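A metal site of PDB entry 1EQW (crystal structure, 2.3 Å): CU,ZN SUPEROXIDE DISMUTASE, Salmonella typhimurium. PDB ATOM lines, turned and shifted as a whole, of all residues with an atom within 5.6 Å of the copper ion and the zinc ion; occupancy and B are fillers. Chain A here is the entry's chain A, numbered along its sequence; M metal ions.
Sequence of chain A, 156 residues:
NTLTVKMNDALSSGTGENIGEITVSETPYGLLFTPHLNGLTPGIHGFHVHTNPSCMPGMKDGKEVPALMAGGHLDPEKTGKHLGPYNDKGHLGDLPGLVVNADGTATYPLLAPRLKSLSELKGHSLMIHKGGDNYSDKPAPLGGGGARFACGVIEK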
ATOM      1  N   PHE A  47       7.664 -30.318  -4.707  1.00  0.00           N
ATOM      2  CA  PHE A  47       8.934 -29.948  -5.337  1.00  0.00           C
ATOM      3  C   PHE A  47       8.824 -30.173  -6.852  1.00  0.00           C
ATOM      4  O   PHE A  47       8.805 -31.318  -7.298  1.00  0.00           O
ATOM      5  CB  PHE A  47      10.054 -30.810  -4.740  1.00  0.00           C
ATOM      6  CG  PHE A  47      11.438 -30.610  -5.281  1.00  0.00           C
ATOM      7  CD1 PHE A  47      11.965 -29.332  -5.460  1.00  0.00           C
ATOM      8  CD2 PHE A  47      12.215 -31.708  -5.612  1.00  0.00           C
ATOM      9  CE1 PHE A  47      13.255 -29.161  -5.958  1.00  0.00           C
ATOM     10  CE2 PHE A  47      13.516 -31.554  -6.111  1.00  0.00           C
ATOM     11  CZ  PHE A  47      14.035 -30.281  -6.289  1.00  0.00           C
ATOM     12  N   HIS A  48       8.776 -29.089  -7.626  1.00  0.00           N
ATOM     13  CA  HIS A  48       8.628 -29.224  -9.076  1.00  0.00           C
ATOM     14  C   HIS A  48       9.470 -28.249  -9.885  1.00  0.00           C
ATOM     15  O   HIS A  48       9.910 -27.215  -9.381  1.00  0.00           O
ATOM     16  CB  HIS A  48       7.188 -29.049  -9.525  1.00  0.00           C
ATOM     17  CG  HIS A  48       6.172 -29.390  -8.434  1.00  0.00           C
ATOM     18  ND1 HIS A  48       5.485 -28.450  -7.708  1.00  0.00           N
ATOM     19  CD2 HIS A  48       5.758 -30.599  -7.990  1.00  0.00           C
ATOM     20  CE1 HIS A  48       4.681 -29.055  -6.862  1.00  0.00           C
ATOM     21  NE2 HIS A  48       4.827 -30.363  -7.004  1.00  0.00           N
ATOM     22  N   HIS A  50       9.517 -25.535 -12.685  1.00  0.00           N
ATOM     23  CA  HIS A  50       8.577 -24.625 -13.317  1.00  0.00           C
ATOM     24  C   HIS A  50       9.126 -24.071 -14.653  1.00  0.00           C
ATOM     25  O   HIS A  50      10.333 -23.972 -14.876  1.00  0.00           O
ATOM     26  CB  HIS A  50       8.211 -23.514 -12.355  1.00  0.00           C
ATOM     27  CG  HIS A  50       7.208 -23.966 -11.264  1.00  0.00           C
ATOM     28  ND1 HIS A  50       6.037 -23.304 -10.972  1.00  0.00           N
ATOM     29  CD2 HIS A  50       7.264 -25.027 -10.410  1.00  0.00           C
ATOM     30  CE1 HIS A  50       5.413 -23.932  -9.987  1.00  0.00           C
ATOM     31  NE2 HIS A  50       6.137 -24.977  -9.626  1.00  0.00           N
ATOM     32  N   HIS A  73       3.889 -25.476 -13.757  1.00  0.00           N
ATOM     33  CA  HIS A  73       4.757 -26.642 -13.776  1.00  0.00           C
ATOM     34  C   HIS A  73       5.174 -26.983 -15.196  1.00  0.00           C
ATOM     35  O   HIS A  73       4.341 -26.967 -16.105  1.00  0.00           O
ATOM     36  CB  HIS A  73       4.038 -27.855 -13.210  1.00  0.00           C
ATOM     37  CG  HIS A  73       3.810 -27.743 -11.709  1.00  0.00           C
ATOM     38  ND1 HIS A  73       3.358 -28.807 -10.950  1.00  0.00           N
ATOM     39  CD2 HIS A  73       3.960 -26.706 -10.854  1.00  0.00           C
ATOM     40  CE1 HIS A  73       3.242 -28.426  -9.692  1.00  0.00           C
ATOM     41  NE2 HIS A  73       3.597 -27.157  -9.605  1.00  0.00           N
ATOM     42  N   LYS A  81      -2.190 -32.183 -16.386  1.00  0.00           N
ATOM     43  CA  LYS A  81      -2.407 -33.081 -15.258  1.00  0.00           C
ATOM     44  C   LYS A  81      -1.151 -33.294 -14.421  1.00  0.00           C
ATOM     45  O   LYS A  81      -0.088 -33.642 -14.937  1.00  0.00           O
ATOM     46  CB  LYS A  81      -2.929 -34.431 -15.775  1.00  0.00           C
ATOM     47  CG  LYS A  81      -4.211 -34.320 -16.586  1.00  0.00           C
ATOM     48  CD  LYS A  81      -4.753 -35.689 -16.999  1.00  0.00           C
ATOM     49  CE  LYS A  81      -6.113 -35.555 -17.669  1.00  0.00           C
ATOM     50  NZ  LYS A  81      -6.654 -36.875 -18.093  1.00  0.00           N
ATOM     51  N   HIS A  82      -1.293 -33.100 -13.115  1.00  0.00           N
ATOM     52  CA  HIS A  82      -0.221 -33.285 -12.173  1.00  0.00           C
ATOM     53  C   HIS A  82      -0.260 -34.688 -11.623  1.00  0.00           C
ATOM     54  O   HIS A  82      -0.988 -34.986 -10.682  1.00  0.00           O
ATOM     55  CB  HIS A  82      -0.353 -32.223 -11.069  1.00  0.00           C
ATOM     56  CG  HIS A  82       0.757 -32.330 -10.013  1.00  0.00           C
ATOM     57  ND1 HIS A  82       2.056 -31.941 -10.275  1.00  0.00           N
ATOM     58  CD2 HIS A  82       0.741 -32.771  -8.740  1.00  0.00           C
ATOM     59  CE1 HIS A  82       2.787 -32.144  -9.186  1.00  0.00           C
ATOM     60  NE2 HIS A  82       2.010 -32.642  -8.245  1.00  0.00           N
ATOM     61  N   LEU A  83       0.567 -35.605 -12.196  1.00  0.00           N
ATOM     62  CA  LEU A  83       0.473 -37.010 -11.780  1.00  0.00           C
ATOM     63  C   LEU A  83       1.737 -37.453 -11.029  1.00  0.00           C
ATOM     64  O   LEU A  83       1.793 -38.651 -10.627  1.00  0.00           O
ATOM     65  CB  LEU A  83       0.254 -37.913 -12.992  1.00  0.00           C
ATOM     66  CG  LEU A  83      -1.022 -37.667 -13.807  1.00  0.00           C
ATOM     67  CD1 LEU A  83      -1.106 -38.639 -14.985  1.00  0.00           C
ATOM     68  CD2 LEU A  83      -2.253 -37.787 -12.935  1.00  0.00           C
ATOM     69  N   HIS A  91       2.742 -33.666 -15.705  1.00  0.00           N
ATOM     70  CA  HIS A  91       3.780 -32.645 -15.795  1.00  0.00           C
ATOM     71  C   HIS A  91       5.174 -33.194 -15.786  1.00  0.00           C
ATOM     72  O   HIS A  91       5.589 -33.800 -14.798  1.00  0.00           O
ATOM     73  CB  HIS A  91       3.651 -31.694 -14.598  1.00  0.00           C
ATOM     74  CG  HIS A  91       2.305 -30.977 -14.506  1.00  0.00           C
ATOM     75  ND1 HIS A  91       1.646 -30.793 -13.303  1.00  0.00           N
ATOM     76  CD2 HIS A  91       1.531 -30.405 -15.455  1.00  0.00           C
ATOM     77  CE1 HIS A  91       0.525 -30.136 -13.522  1.00  0.00           C
ATOM     78  NE2 HIS A  91       0.425 -29.890 -14.815  1.00  0.00           N
ATOM     79  N   GLY A  93       7.723 -31.771 -15.307  1.00  0.00           N
ATOM     80  CA  GLY A  93       8.419 -31.086 -14.224  1.00  0.00           C
ATOM     81  C   GLY A  93       8.120 -31.623 -12.841  1.00  0.00           C
ATOM     82  O   GLY A  93       8.662 -31.128 -11.854  1.00  0.00           O
ATOM     83  N   ASP A  94       7.259 -32.636 -12.745  1.00  0.00           N
ATOM     84  CA  ASP A  94       6.888 -33.191 -11.442  1.00  0.00           C
ATOM     85  C   ASP A  94       7.999 -34.035 -10.824  1.00  0.00           C
ATOM     86  O   ASP A  94       8.308 -35.132 -11.295  1.00  0.00           O
ATOM     87  CB  ASP A  94       5.617 -34.038 -11.578  1.00  0.00           C
ATOM     88  CG  ASP A  94       4.364 -33.195 -11.764  1.00  0.00           C
ATOM     89  OD1 ASP A  94       4.472 -31.952 -11.745  1.00  0.00           O
ATOM     90  OD2 ASP A  94       3.271 -33.769 -11.919  1.00  0.00           O
ATOM     91  N   MET A 127      11.108 -25.323  -7.816  1.00  0.00           N
ATOM     92  CA  MET A 127      10.211 -24.754  -6.821  1.00  0.00           C
ATOM     93  C   MET A 127       9.932 -25.650  -5.614  1.00  0.00           C
ATOM     94  O   MET A 127       9.777 -26.867  -5.749  1.00  0.00           O
ATOM     95  CB  MET A 127       8.873 -24.414  -7.479  1.00  0.00           C
ATOM     96  CG  MET A 127       8.059 -23.368  -6.728  1.00  0.00           C
ATOM     97  SD  MET A 127       8.463 -21.683  -7.222  1.00  0.00           S
ATOM     98  CE  MET A 127       7.531 -20.743  -6.020  1.00  0.00           C
ATOM     99  N   HIS A 129       7.249 -25.738  -2.543  1.00  0.00           N
ATOM    100  CA  HIS A 129       5.996 -25.179  -2.036  1.00  0.00           C
ATOM    101  C   HIS A 129       5.859 -25.330  -0.531  1.00  0.00           C
ATOM    102  O   HIS A 129       6.658 -26.009   0.104  1.00  0.00           O
ATOM    103  CB  HIS A 129       4.822 -25.869  -2.693  1.00  0.00           C
ATOM    104  CG  HIS A 129       4.776 -25.681  -4.214  1.00  0.00           C
ATOM    105  ND1 HIS A 129       3.920 -24.801  -4.826  1.00  0.00           N
ATOM    106  CD2 HIS A 129       5.507 -26.252  -5.196  1.00  0.00           C
ATOM    107  CE1 HIS A 129       4.116 -24.840  -6.133  1.00  0.00           C
ATOM    108  NE2 HIS A 129       5.072 -25.717  -6.392  1.00  0.00           N
ATOM    109  N   LEU A 142      -2.799 -29.765  -8.125  1.00  0.00           N
ATOM    110  CA  LEU A 142      -1.339 -29.724  -8.047  1.00  0.00           C
ATOM    111  C   LEU A 142      -0.779 -30.338  -6.766  1.00  0.00           C
ATOM    112  O   LEU A 142       0.040 -29.740  -6.060  1.00  0.00           O
ATOM    113  CB  LEU A 142      -0.868 -28.258  -8.172  1.00  0.00           C
ATOM    114  CG  LEU A 142      -0.739 -27.652  -9.575  1.00  0.00           C
ATOM    115  CD1 LEU A 142      -1.677 -28.347 -10.545  1.00  0.00           C
ATOM    116  CD2 LEU A 142      -1.006 -26.166  -9.531  1.00  0.00           C
HETATM  117 CU    CU M   1       5.405 -26.219  -8.211  1.00  0.00          CU
HETATM  118 ZN    ZN M   2       2.759 -30.738 -11.575  1.00  0.00          ZN
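Residues that only touch the copper ion: Met 127. Five residues have an atom within 4 Å of the copper ion: His 48, His 50, His 73, Met 127 and His 129.
O of Lys 81 lies within hydrogen-bond range of N of His 91, 2.9 Å away. OD2 of Asp 94 is in hydrogen-bond range of N of Leu 83, 3.3 Å away. The backbone NH (N) of Met 127 sits at hydrogen-bond distance from the backbone carbonyl oxygen (O) of His 48 (2.7 Å).
Within 4 Å of the zinc ion: His 73, His 82, His 91 and Asp 94. The nearest printed residue that does not touch the zinc ion is His 48 (4.7 Å).
The copper ion is bound by NE2 of His 129 (1.9 Å). NE2 of His 50 is bound to the copper ion, 2.0 Å away. The copper ion is bound by ND1 of His 48 (2.3 Å). The copper ion is bound by NE2 of His 73, 2.5 Å away. The copper ion has four donor atoms within binding distance.
A ring nitrogen (ND1) of His 82 binds the zinc ion (1.9 Å). The zinc ion is bound by a ring nitrogen (ND1) of His 91 (2.1 Å). The zinc ion is bound by the side-chain carboxylate (OD1) of Asp 94. ND1 of His 73 is bound to the zinc ion, at 2.1 Å. The zinc ion has four donor atoms within binding distance.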
